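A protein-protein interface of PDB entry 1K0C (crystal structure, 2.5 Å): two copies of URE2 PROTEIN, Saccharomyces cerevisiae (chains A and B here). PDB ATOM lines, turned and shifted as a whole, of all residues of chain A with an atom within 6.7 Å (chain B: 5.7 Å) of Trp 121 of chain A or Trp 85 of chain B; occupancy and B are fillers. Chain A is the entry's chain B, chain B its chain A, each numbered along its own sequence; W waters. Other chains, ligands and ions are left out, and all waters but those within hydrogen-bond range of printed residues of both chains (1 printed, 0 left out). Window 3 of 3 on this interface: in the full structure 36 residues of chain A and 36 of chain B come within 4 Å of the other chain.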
ATOM      1  N   SER A 116     -21.210  20.007 -14.749  1.00  0.00           N
ATOM      2  CA  SER A 116     -20.692  21.283 -14.294  1.00  0.00           C
ATOM      3  C   SER A 116     -19.414  21.008 -13.521  1.00  0.00           C
ATOM      4  O   SER A 116     -18.475  21.797 -13.552  1.00  0.00           O
ATOM      5  CB  SER A 116     -21.713  22.008 -13.411  1.00  0.00           C
ATOM      6  OG  SER A 116     -21.825  21.404 -12.133  1.00  0.00           O
ATOM      7  N   GLN A 117     -19.378  19.880 -12.827  1.00  0.00           N
ATOM      8  CA  GLN A 117     -18.192  19.502 -12.071  1.00  0.00           C
ATOM      9  C   GLN A 117     -17.074  19.089 -13.025  1.00  0.00           C
ATOM     10  O   GLN A 117     -15.929  19.505 -12.869  1.00  0.00           O
ATOM     11  CB  GLN A 117     -18.521  18.364 -11.101  1.00  0.00           C
ATOM     12  CG  GLN A 117     -19.408  18.815  -9.966  1.00  0.00           C
ATOM     13  CD  GLN A 117     -18.782  19.962  -9.192  1.00  0.00           C
ATOM     14  OE1 GLN A 117     -19.482  20.798  -8.618  1.00  0.00           O
ATOM     15  NE2 GLN A 117     -17.447  20.001  -9.167  1.00  0.00           N
ATOM     16  N   ILE A 118     -17.411  18.276 -14.019  1.00  0.00           N
ATOM     17  CA  ILE A 118     -16.427  17.849 -14.996  1.00  0.00           C
ATOM     18  C   ILE A 118     -15.844  19.070 -15.709  1.00  0.00           C
ATOM     19  O   ILE A 118     -14.623  19.202 -15.829  1.00  0.00           O
ATOM     20  CB  ILE A 118     -17.054  16.886 -16.013  1.00  0.00           C
ATOM     21  CG1 ILE A 118     -17.431  15.577 -15.313  1.00  0.00           C
ATOM     22  CG2 ILE A 118     -16.084  16.620 -17.154  1.00  0.00           C
ATOM     23  CD1 ILE A 118     -18.268  14.640 -16.167  1.00  0.00           C
ATOM     24  N   ASN A 119     -16.704  19.974 -16.166  1.00  0.00           N
ATOM     25  CA  ASN A 119     -16.224  21.177 -16.841  1.00  0.00           C
ATOM     26  C   ASN A 119     -15.275  22.014 -15.971  1.00  0.00           C
ATOM     27  O   ASN A 119     -14.279  22.549 -16.462  1.00  0.00           O
ATOM     28  CB  ASN A 119     -17.405  22.030 -17.280  1.00  0.00           C
ATOM     29  CG  ASN A 119     -18.183  21.397 -18.407  1.00  0.00           C
ATOM     30  OD1 ASN A 119     -19.358  21.697 -18.614  1.00  0.00           O
ATOM     31  ND2 ASN A 119     -17.528  20.521 -19.155  1.00  0.00           N
ATOM     32  N   ALA A 120     -15.584  22.124 -14.682  1.00  0.00           N
ATOM     33  CA  ALA A 120     -14.764  22.899 -13.758  1.00  0.00           C
ATOM     34  C   ALA A 120     -13.312  22.431 -13.808  1.00  0.00           C
ATOM     35  O   ALA A 120     -12.396  23.233 -14.031  1.00  0.00           O
ATOM     36  CB  ALA A 120     -15.312  22.768 -12.338  1.00  0.00           C
ATOM     37  N   TRP A 121     -13.111  21.131 -13.596  1.00  0.00           N
ATOM     38  CA  TRP A 121     -11.776  20.551 -13.626  1.00  0.00           C
ATOM     39  C   TRP A 121     -11.175  20.692 -15.016  1.00  0.00           C
ATOM     40  O   TRP A 121      -9.960  20.850 -15.165  1.00  0.00           O
ATOM     41  CB  TRP A 121     -11.809  19.064 -13.225  1.00  0.00           C
ATOM     42  CG  TRP A 121     -12.130  18.839 -11.765  1.00  0.00           C
ATOM     43  CD1 TRP A 121     -13.327  18.424 -11.236  1.00  0.00           C
ATOM     44  CD2 TRP A 121     -11.275  19.124 -10.643  1.00  0.00           C
ATOM     45  NE1 TRP A 121     -13.269  18.444  -9.858  1.00  0.00           N
ATOM     46  CE2 TRP A 121     -12.025  18.873  -9.468  1.00  0.00           C
ATOM     47  CE3 TRP A 121      -9.955  19.575 -10.517  1.00  0.00           C
ATOM     48  CZ2 TRP A 121     -11.495  19.064  -8.179  1.00  0.00           C
ATOM     49  CZ3 TRP A 121      -9.424  19.766  -9.228  1.00  0.00           C
ATOM     50  CH2 TRP A 121     -10.202  19.510  -8.080  1.00  0.00           C
ATOM     51  N   LEU A 122     -12.027  20.644 -16.035  1.00  0.00           N
ATOM     52  CA  LEU A 122     -11.553  20.748 -17.404  1.00  0.00           C
ATOM     53  C   LEU A 122     -11.020  22.151 -17.698  1.00  0.00           C
ATOM     54  O   LEU A 122      -9.896  22.301 -18.193  1.00  0.00           O
ATOM     55  CB  LEU A 122     -12.672  20.383 -18.380  1.00  0.00           C
ATOM     56  CG  LEU A 122     -12.255  20.364 -19.857  1.00  0.00           C
ATOM     57  CD1 LEU A 122     -11.009  19.498 -20.071  1.00  0.00           C
ATOM     58  CD2 LEU A 122     -13.420  19.844 -20.682  1.00  0.00           C
ATOM     59  N   PHE A 123     -11.810  23.175 -17.390  1.00  0.00           N
ATOM     60  CA  PHE A 123     -11.360  24.546 -17.622  1.00  0.00           C
ATOM     61  C   PHE A 123     -10.156  24.853 -16.722  1.00  0.00           C
ATOM     62  O   PHE A 123      -9.229  25.559 -17.117  1.00  0.00           O
ATOM     63  CB  PHE A 123     -12.499  25.553 -17.372  1.00  0.00           C
ATOM     64  CG  PHE A 123     -13.351  25.817 -18.588  1.00  0.00           C
ATOM     65  CD1 PHE A 123     -14.533  25.119 -18.797  1.00  0.00           C
ATOM     66  CD2 PHE A 123     -12.939  26.737 -19.549  1.00  0.00           C
ATOM     67  CE1 PHE A 123     -15.294  25.325 -19.938  1.00  0.00           C
ATOM     68  CE2 PHE A 123     -13.695  26.953 -20.701  1.00  0.00           C
ATOM     69  CZ  PHE A 123     -14.875  26.245 -20.896  1.00  0.00           C
ATOM     70  N   PHE A 124     -10.169  24.315 -15.513  1.00  0.00           N
ATOM     71  CA  PHE A 124      -9.054  24.524 -14.611  1.00  0.00           C
ATOM     72  C   PHE A 124      -7.779  23.933 -15.222  1.00  0.00           C
ATOM     73  O   PHE A 124      -6.707  24.514 -15.126  1.00  0.00           O
ATOM     74  CB  PHE A 124      -9.341  23.861 -13.272  1.00  0.00           C
ATOM     75  CG  PHE A 124      -8.203  23.950 -12.301  1.00  0.00           C
ATOM     76  CD1 PHE A 124      -7.571  25.170 -12.063  1.00  0.00           C
ATOM     77  CD2 PHE A 124      -7.787  22.828 -11.596  1.00  0.00           C
ATOM     78  CE1 PHE A 124      -6.536  25.269 -11.127  1.00  0.00           C
ATOM     79  CE2 PHE A 124      -6.760  22.915 -10.661  1.00  0.00           C
ATOM     80  CZ  PHE A 124      -6.132  24.141 -10.424  1.00  0.00           C
ATOM     81  N   GLN A 125      -7.901  22.775 -15.856  1.00  0.00           N
ATOM     82  CA  GLN A 125      -6.754  22.132 -16.476  1.00  0.00           C
ATOM     83  C   GLN A 125      -6.264  22.958 -17.663  1.00  0.00           C
ATOM     84  O   GLN A 125      -5.073  23.247 -17.777  1.00  0.00           O
ATOM     85  CB  GLN A 125      -7.139  20.717 -16.936  1.00  0.00           C
ATOM     86  CG  GLN A 125      -5.968  19.778 -17.212  1.00  0.00           C
ATOM     87  CD  GLN A 125      -5.187  20.153 -18.460  1.00  0.00           C
ATOM     88  OE1 GLN A 125      -4.059  20.657 -18.380  1.00  0.00           O
ATOM     89  NE2 GLN A 125      -5.788  19.917 -19.627  1.00  0.00           N
ATOM     90  N   THR A 126      -7.180  23.350 -18.542  1.00  0.00           N
ATOM     91  CA  THR A 126      -6.808  24.132 -19.721  1.00  0.00           C
ATOM     92  C   THR A 126      -6.452  25.597 -19.428  1.00  0.00           C
ATOM     93  O   THR A 126      -5.647  26.200 -20.133  1.00  0.00           O
ATOM     94  CB  THR A 126      -7.936  24.122 -20.788  1.00  0.00           C
ATOM     95  OG1 THR A 126      -9.118  24.722 -20.241  1.00  0.00           O
ATOM     96  CG2 THR A 126      -8.246  22.698 -21.234  1.00  0.00           C
ATOM     97  N   VAL A 161      -1.243  24.546  -8.124  1.00  0.00           N
ATOM     98  CA  VAL A 161      -2.358  23.897  -8.796  1.00  0.00           C
ATOM     99  C   VAL A 161      -2.352  22.399  -8.558  1.00  0.00           C
ATOM    100  O   VAL A 161      -3.415  21.796  -8.430  1.00  0.00           O
ATOM    101  CB  VAL A 161      -2.367  24.181 -10.314  1.00  0.00           C
ATOM    102  CG1 VAL A 161      -2.097  25.654 -10.557  1.00  0.00           C
ATOM    103  CG2 VAL A 161      -1.348  23.333 -11.027  1.00  0.00           C
ATOM    104  N   VAL A 164      -4.042  21.544  -5.255  1.00  0.00           N
ATOM    105  CA  VAL A 164      -5.500  21.530  -5.271  1.00  0.00           C
ATOM    106  C   VAL A 164      -6.007  20.170  -5.736  1.00  0.00           C
ATOM    107  O   VAL A 164      -6.975  19.638  -5.194  1.00  0.00           O
ATOM    108  CB  VAL A 164      -6.044  22.617  -6.219  1.00  0.00           C
ATOM    109  CG1 VAL A 164      -7.555  22.511  -6.326  1.00  0.00           C
ATOM    110  CG2 VAL A 164      -5.614  24.004  -5.714  1.00  0.00           C
ATOM    111  N   VAL A 165      -5.351  19.614  -6.749  1.00  0.00           N
ATOM    112  CA  VAL A 165      -5.736  18.312  -7.267  1.00  0.00           C
ATOM    113  C   VAL A 165      -5.448  17.244  -6.221  1.00  0.00           C
ATOM    114  O   VAL A 165      -6.267  16.355  -5.977  1.00  0.00           O
ATOM    115  CB  VAL A 165      -4.956  17.956  -8.552  1.00  0.00           C
ATOM    116  CG1 VAL A 165      -5.343  16.566  -9.021  1.00  0.00           C
ATOM    117  CG2 VAL A 165      -5.238  18.981  -9.642  1.00  0.00           C
ATOM    118  N   ALA A 168      -7.862  17.443  -3.416  1.00  0.00           N
ATOM    119  CA  ALA A 168      -9.153  16.949  -3.882  1.00  0.00           C
ATOM    120  C   ALA A 168      -9.163  15.423  -3.891  1.00  0.00           C
ATOM    121  O   ALA A 168     -10.104  14.802  -3.401  1.00  0.00           O
ATOM    122  CB  ALA A 168      -9.453  17.485  -5.286  1.00  0.00           C
ATOM    123  N   LEU A 169      -8.118  14.827  -4.458  1.00  0.00           N
ATOM    124  CA  LEU A 169      -8.015  13.378  -4.513  1.00  0.00           C
ATOM    125  C   LEU A 169      -7.981  12.798  -3.101  1.00  0.00           C
ATOM    126  O   LEU A 169      -8.709  11.850  -2.789  1.00  0.00           O
ATOM    127  CB  LEU A 169      -6.758  12.961  -5.280  1.00  0.00           C
ATOM    128  CG  LEU A 169      -6.812  13.152  -6.799  1.00  0.00           C
ATOM    129  CD1 LEU A 169      -5.491  12.717  -7.412  1.00  0.00           C
ATOM    130  CD2 LEU A 169      -7.968  12.338  -7.387  1.00  0.00           C
ATOM    131  N   ARG A 172     -11.377  12.803  -1.710  1.00  0.00           N
ATOM    132  CA  ARG A 172     -12.246  11.769  -2.261  1.00  0.00           C
ATOM    133  C   ARG A 172     -11.961  10.438  -1.567  1.00  0.00           C
ATOM    134  O   ARG A 172     -12.879   9.700  -1.212  1.00  0.00           O
ATOM    135  CB  ARG A 172     -12.006  11.612  -3.762  1.00  0.00           C
ATOM    136  CG  ARG A 172     -12.277  12.848  -4.598  1.00  0.00           C
ATOM    137  CD  ARG A 172     -13.756  13.039  -4.876  1.00  0.00           C
ATOM    138  NE  ARG A 172     -13.975  14.122  -5.831  1.00  0.00           N
ATOM    139  CZ  ARG A 172     -13.638  15.389  -5.607  1.00  0.00           C
ATOM    140  NH1 ARG A 172     -13.073  15.728  -4.455  1.00  0.00           N
ATOM    141  NH2 ARG A 172     -13.852  16.317  -6.536  1.00  0.00           N
ATOM    142  N   LEU A 207     -11.893  12.404  -9.772  1.00  0.00           N
ATOM    143  CA  LEU A 207     -12.365  13.760  -9.530  1.00  0.00           C
ATOM    144  C   LEU A 207     -13.885  13.927  -9.453  1.00  0.00           C
ATOM    145  O   LEU A 207     -14.385  14.623  -8.575  1.00  0.00           O
ATOM    146  CB  LEU A 207     -11.783  14.692 -10.596  1.00  0.00           C
ATOM    147  CG  LEU A 207     -10.252  14.695 -10.580  1.00  0.00           C
ATOM    148  CD1 LEU A 207      -9.712  15.411 -11.803  1.00  0.00           C
ATOM    149  CD2 LEU A 207      -9.766  15.354  -9.303  1.00  0.00           C
ATOM    150  N   VAL A 208     -14.625  13.289 -10.353  1.00  0.00           N
ATOM    151  CA  VAL A 208     -16.072  13.441 -10.338  1.00  0.00           C
ATOM    152  C   VAL A 208     -16.846  12.129 -10.403  1.00  0.00           C
ATOM    153  O   VAL A 208     -16.464  11.198 -11.125  1.00  0.00           O
ATOM    154  CB  VAL A 208     -16.543  14.361 -11.514  1.00  0.00           C
ATOM    155  CG1 VAL A 208     -18.068  14.463 -11.533  1.00  0.00           C
ATOM    156  CG2 VAL A 208     -15.931  15.752 -11.369  1.00  0.00           C
ATOM    157  N   ALA A 215     -12.342  14.570 -17.090  1.00  0.00           N
ATOM    158  CA  ALA A 215     -11.772  15.411 -16.043  1.00  0.00           C
ATOM    159  C   ALA A 215     -10.417  14.865 -15.601  1.00  0.00           C
ATOM    160  O   ALA A 215      -9.430  15.597 -15.551  1.00  0.00           O
ATOM    161  CB  ALA A 215     -12.717  15.474 -14.844  1.00  0.00           C
ATOM    162  N   ASP A 216     -10.377  13.575 -15.287  1.00  0.00           N
ATOM    163  CA  ASP A 216      -9.147  12.932 -14.839  1.00  0.00           C
ATOM    164  C   ASP A 216      -8.116  12.826 -15.951  1.00  0.00           C
ATOM    165  O   ASP A 216      -6.938  13.140 -15.753  1.00  0.00           O
ATOM    166  CB  ASP A 216      -9.457  11.537 -14.308  1.00  0.00           C
ATOM    167  CG  ASP A 216     -10.567  11.544 -13.281  1.00  0.00           C
ATOM    168  OD1 ASP A 216     -10.299  11.941 -12.127  1.00  0.00           O
ATOM    169  OD2 ASP A 216     -11.712  11.170 -13.629  1.00  0.00           O
ATOM    170  N   ALA A 218      -7.623  14.584 -18.792  1.00  0.00           N
ATOM    171  CA  ALA A 218      -7.017  15.823 -19.266  1.00  0.00           C
ATOM    172  C   ALA A 218      -5.647  16.080 -18.649  1.00  0.00           C
ATOM    173  O   ALA A 218      -4.772  16.659 -19.293  1.00  0.00           O
ATOM    174  CB  ALA A 218      -7.944  16.996 -18.985  1.00  0.00           C
ATOM    175  N   PHE A 219      -5.452  15.641 -17.408  1.00  0.00           N
ATOM    176  CA  PHE A 219      -4.179  15.872 -16.728  1.00  0.00           C
ATOM    177  C   PHE A 219      -3.050  14.908 -17.085  1.00  0.00           C
ATOM    178  O   PHE A 219      -1.880  15.254 -16.949  1.00  0.00           O
ATOM    179  CB  PHE A 219      -4.374  15.843 -15.207  1.00  0.00           C
ATOM    180  CG  PHE A 219      -5.256  16.941 -14.678  1.00  0.00           C
ATOM    181  CD1 PHE A 219      -6.637  16.823 -14.718  1.00  0.00           C
ATOM    182  CD2 PHE A 219      -4.699  18.088 -14.113  1.00  0.00           C
ATOM    183  CE1 PHE A 219      -7.454  17.826 -14.201  1.00  0.00           C
ATOM    184  CE2 PHE A 219      -5.502  19.093 -13.598  1.00  0.00           C
ATOM    185  CZ  PHE A 219      -6.886  18.962 -13.639  1.00  0.00           C
ATOM    186  N   VAL B  65     -16.372  25.829  -1.844  1.00  0.00           N
ATOM    187  CA  VAL B  65     -17.088  26.230  -3.042  1.00  0.00           C
ATOM    188  C   VAL B  65     -16.127  26.152  -4.227  1.00  0.00           C
ATOM    189  O   VAL B  65     -16.498  25.670  -5.299  1.00  0.00           O
ATOM    190  CB  VAL B  65     -17.646  27.663  -2.901  1.00  0.00           C
ATOM    191  CG1 VAL B  65     -18.281  28.115  -4.206  1.00  0.00           C
ATOM    192  CG2 VAL B  65     -18.674  27.700  -1.790  1.00  0.00           C
ATOM    193  N   ASN B  66     -14.894  26.621  -4.022  1.00  0.00           N
ATOM    194  CA  ASN B  66     -13.864  26.580  -5.059  1.00  0.00           C
ATOM    195  C   ASN B  66     -12.505  26.117  -4.503  1.00  0.00           C
ATOM    196  O   ASN B  66     -11.770  26.894  -3.880  1.00  0.00           O
ATOM    197  CB  ASN B  66     -13.701  27.953  -5.711  1.00  0.00           C
ATOM    198  CG  ASN B  66     -12.735  27.925  -6.892  1.00  0.00           C
ATOM    199  OD1 ASN B  66     -12.542  28.933  -7.579  1.00  0.00           O
ATOM    200  ND2 ASN B  66     -12.125  26.764  -7.134  1.00  0.00           N
ATOM    201  N   PRO B  67     -12.149  24.844  -4.729  1.00  0.00           N
ATOM    202  CA  PRO B  67     -10.864  24.356  -4.222  1.00  0.00           C
ATOM    203  C   PRO B  67      -9.668  25.144  -4.742  1.00  0.00           C
ATOM    204  O   PRO B  67      -8.614  25.165  -4.104  1.00  0.00           O
ATOM    205  CB  PRO B  67     -10.844  22.892  -4.667  1.00  0.00           C
ATOM    206  CG  PRO B  67     -11.692  22.894  -5.901  1.00  0.00           C
ATOM    207  CD  PRO B  67     -12.843  23.798  -5.500  1.00  0.00           C
ATOM    208  N   ASN B  68      -9.833  25.798  -5.891  1.00  0.00           N
ATOM    209  CA  ASN B  68      -8.750  26.583  -6.488  1.00  0.00           C
ATOM    210  C   ASN B  68      -8.585  27.945  -5.791  1.00  0.00           C
ATOM    211  O   ASN B  68      -7.676  28.712  -6.117  1.00  0.00           O
ATOM    212  CB  ASN B  68      -9.019  26.792  -7.984  1.00  0.00           C
ATOM    213  CG  ASN B  68      -7.823  27.384  -8.723  1.00  0.00           C
ATOM    214  OD1 ASN B  68      -7.979  28.246  -9.591  1.00  0.00           O
ATOM    215  ND2 ASN B  68      -6.627  26.916  -8.393  1.00  0.00           N
ATOM    216  N   PRO B  72     -14.203  33.807 -10.373  1.00  0.00           N
ATOM    217  CA  PRO B  72     -15.470  33.634  -9.661  1.00  0.00           C
ATOM    218  C   PRO B  72     -15.886  32.203  -9.334  1.00  0.00           C
ATOM    219  O   PRO B  72     -15.371  31.229  -9.895  1.00  0.00           O
ATOM    220  CB  PRO B  72     -16.465  34.282 -10.605  1.00  0.00           C
ATOM    221  CG  PRO B  72     -15.966  33.773 -11.929  1.00  0.00           C
ATOM    222  CD  PRO B  72     -14.446  33.954 -11.823  1.00  0.00           C
ATOM    223  N   ALA B  73     -16.840  32.108  -8.411  1.00  0.00           N
ATOM    224  CA  ALA B  73     -17.436  30.849  -7.999  1.00  0.00           C
ATOM    225  C   ALA B  73     -18.930  31.160  -8.002  1.00  0.00           C
ATOM    226  O   ALA B  73     -19.335  32.325  -7.902  1.00  0.00           O
ATOM    227  CB  ALA B  73     -16.964  30.451  -6.617  1.00  0.00           C
ATOM    228  N   LEU B  74     -19.755  30.134  -8.135  1.00  0.00           N
ATOM    229  CA  LEU B  74     -21.189  30.356  -8.183  1.00  0.00           C
ATOM    230  C   LEU B  74     -21.971  29.256  -7.491  1.00  0.00           C
ATOM    231  O   LEU B  74     -21.646  28.069  -7.624  1.00  0.00           O
ATOM    232  CB  LEU B  74     -21.653  30.441  -9.635  1.00  0.00           C
ATOM    233  CG  LEU B  74     -23.151  30.658  -9.824  1.00  0.00           C
ATOM    234  CD1 LEU B  74     -23.406  32.161  -9.837  1.00  0.00           C
ATOM    235  CD2 LEU B  74     -23.635  30.040 -11.128  1.00  0.00           C
ATOM    236  N   SER B  83     -22.251  23.946  -6.166  1.00  0.00           N
ATOM    237  CA  SER B  83     -21.113  24.842  -6.251  1.00  0.00           C
ATOM    238  C   SER B  83     -20.465  24.705  -7.638  1.00  0.00           C
ATOM    239  O   SER B  83     -20.238  23.595  -8.118  1.00  0.00           O
ATOM    240  CB  SER B  83     -20.116  24.483  -5.148  1.00  0.00           C
ATOM    241  OG  SER B  83     -19.222  25.547  -4.909  1.00  0.00           O
ATOM    242  N   ILE B  84     -20.180  25.824  -8.292  1.00  0.00           N
ATOM    243  CA  ILE B  84     -19.568  25.760  -9.612  1.00  0.00           C
ATOM    244  C   ILE B  84     -18.450  26.777  -9.731  1.00  0.00           C
ATOM    245  O   ILE B  84     -18.673  27.966  -9.518  1.00  0.00           O
ATOM    246  CB  ILE B  84     -20.585  26.054 -10.721  1.00  0.00           C
ATOM    247  CG1 ILE B  84     -21.851  25.238 -10.501  1.00  0.00           C
ATOM    248  CG2 ILE B  84     -19.985  25.702 -12.072  1.00  0.00           C
ATOM    249  CD1 ILE B  84     -23.054  25.830 -11.172  1.00  0.00           C
ATOM    250  N   TRP B  85     -17.251  26.312 -10.075  1.00  0.00           N
ATOM    251  CA  TRP B  85     -16.115  27.213 -10.223  1.00  0.00           C
ATOM    252  C   TRP B  85     -15.531  27.195 -11.641  1.00  0.00           C
ATOM    253  O   TRP B  85     -15.821  26.295 -12.438  1.00  0.00           O
ATOM    254  CB  TRP B  85     -15.043  26.891  -9.184  1.00  0.00           C
ATOM    255  CG  TRP B  85     -14.749  25.438  -9.061  1.00  0.00           C
ATOM    256  CD1 TRP B  85     -15.594  24.465  -8.608  1.00  0.00           C
ATOM    257  CD2 TRP B  85     -13.516  24.786  -9.381  1.00  0.00           C
ATOM    258  NE1 TRP B  85     -14.963  23.251  -8.622  1.00  0.00           N
ATOM    259  CE2 TRP B  85     -13.685  23.414  -9.091  1.00  0.00           C
ATOM    260  CE3 TRP B  85     -12.283  25.228  -9.883  1.00  0.00           C
ATOM    261  CZ2 TRP B  85     -12.663  22.473  -9.282  1.00  0.00           C
ATOM    262  CZ3 TRP B  85     -11.261  24.290 -10.074  1.00  0.00           C
ATOM    263  CH2 TRP B  85     -11.460  22.929  -9.772  1.00  0.00           C
ATOM    264  N   GLU B  86     -14.696  28.195 -11.925  1.00  0.00           N
ATOM    265  CA  GLU B  86     -14.090  28.402 -13.245  1.00  0.00           C
ATOM    266  C   GLU B  86     -15.166  29.030 -14.130  1.00  0.00           C
ATOM    267  O   GLU B  86     -16.183  28.396 -14.439  1.00  0.00           O
ATOM    268  CB  GLU B  86     -13.598  27.088 -13.856  1.00  0.00           C
ATOM    269  CG  GLU B  86     -12.248  26.664 -13.348  1.00  0.00           C
ATOM    270  CD  GLU B  86     -11.144  27.575 -13.825  1.00  0.00           C
ATOM    271  OE1 GLU B  86     -10.153  27.736 -13.094  1.00  0.00           O
ATOM    272  OE2 GLU B  86     -11.255  28.121 -14.940  1.00  0.00           O
ATOM    273  N   SER B  87     -14.940  30.287 -14.501  1.00  0.00           N
ATOM    274  CA  SER B  87     -15.875  31.041 -15.335  1.00  0.00           C
ATOM    275  C   SER B  87     -16.354  30.303 -16.592  1.00  0.00           C
ATOM    276  O   SER B  87     -17.516  30.436 -16.990  1.00  0.00           O
ATOM    277  CB  SER B  87     -15.255  32.389 -15.728  1.00  0.00           C
ATOM    278  OG  SER B  87     -14.060  32.215 -16.462  1.00  0.00           O
ATOM    279  N   ALA B  89     -16.724  27.029 -16.999  1.00  0.00           N
ATOM    280  CA  ALA B  89     -17.695  26.011 -16.602  1.00  0.00           C
ATOM    281  C   ALA B  89     -19.016  26.639 -16.145  1.00  0.00           C
ATOM    282  O   ALA B  89     -20.095  26.085 -16.391  1.00  0.00           O
ATOM    283  CB  ALA B  89     -17.102  25.112 -15.499  1.00  0.00           C
ATOM    284  N   ILE B  90     -18.933  27.788 -15.480  1.00  0.00           N
ATOM    285  CA  ILE B  90     -20.131  28.471 -15.013  1.00  0.00           C
ATOM    286  C   ILE B  90     -20.963  28.932 -16.215  1.00  0.00           C
ATOM    287  O   ILE B  90     -22.195  28.823 -16.199  1.00  0.00           O
ATOM    288  CB  ILE B  90     -19.759  29.684 -14.120  1.00  0.00           C
ATOM    289  CG1 ILE B  90     -19.084  29.179 -12.840  1.00  0.00           C
ATOM    290  CG2 ILE B  90     -21.007  30.504 -13.774  1.00  0.00           C
ATOM    291  CD1 ILE B  90     -18.392  30.253 -12.051  1.00  0.00           C
HETATM  292  O   HOH W   1     -20.787  23.155 -16.928  1.00  0.00           O
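O of Ser 83 of chain B sits close to OE1 of Gln 117 of chain A (2.9 Å).
Trp 121 of chain A touches just one residue of chain B: Trp 85 (3.7 Å).
Trp 85 of chain B touches just these residues of chain A: Ala 120, Trp 121 and Phe 124.
Printed residues of chain B within 4 Å of Gln 117 of chain A: Ser 83.
Of the printed residues of chain A, Ser 83 of chain B touches Gln 117 (2.9 Å).
Of the printed residues of chain B, Asn 119 of chain A touches Ala 89 (3.6 Å).
The nearest residue of chain A that does not touch Trp 85 of chain B is Gln 117 of chain A (4.1 Å).
The nearest printed residue of chain A that does not touch Glu 86 of chain B is Asn 119 of chain A (5.3 Å).
Water W1 bridges OD1 of Asn 119 of chain A and O of Ala 89 of chain B.
No position is printed for both chains.
Of the 12 pairs that touch across the chains among the printed residues, none has its exchanged pair printed and touching as well.
The backbone carbonyl oxygen (O) of Val 65 of chain B lies within hydrogen-bond range of the side-chain hydroxyl (OG) of Ser 83 of chain B, 2.8 Å away.
The side-chain hydroxyl of Thr 126 of chain A lies within hydrogen-bond range of the backbone carbonyl oxygen of Phe 123 of chain A, at 3.2 Å.
The side-chain amide nitrogen of Asn 66 of chain B lies close to the backbone NH of Asn 68 of chain B, 2.8 Å away.
Among the printed residues, pairs that only touch across the chains: Phe 124 of chain A with Asn 68 of chain B, Phe 123 of chain A with Ala 89 of chain B, Ala 120 of chain A with Ala 89 of chain B, Ala 120 of chain A with Glu 86 of chain B, Ala 120 of chain A with Trp 85 of chain B, Asn 119 of chain A with Ala 89 of chain B, Val 164 of chain A with Pro 67 of chain B, Trp 121 of chain A with Trp 85 of chain B, Phe 124 of chain A with Glu 86 of chain B, Phe 123 of chain A with Glu 86 of chain B and Phe 124 of chain A with Trp 85 of chain B.
Among the printed residues, no Asp or Glu carboxylate lies within 4 Å of a Lys or Arg side-chain nitrogen of the other chain.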
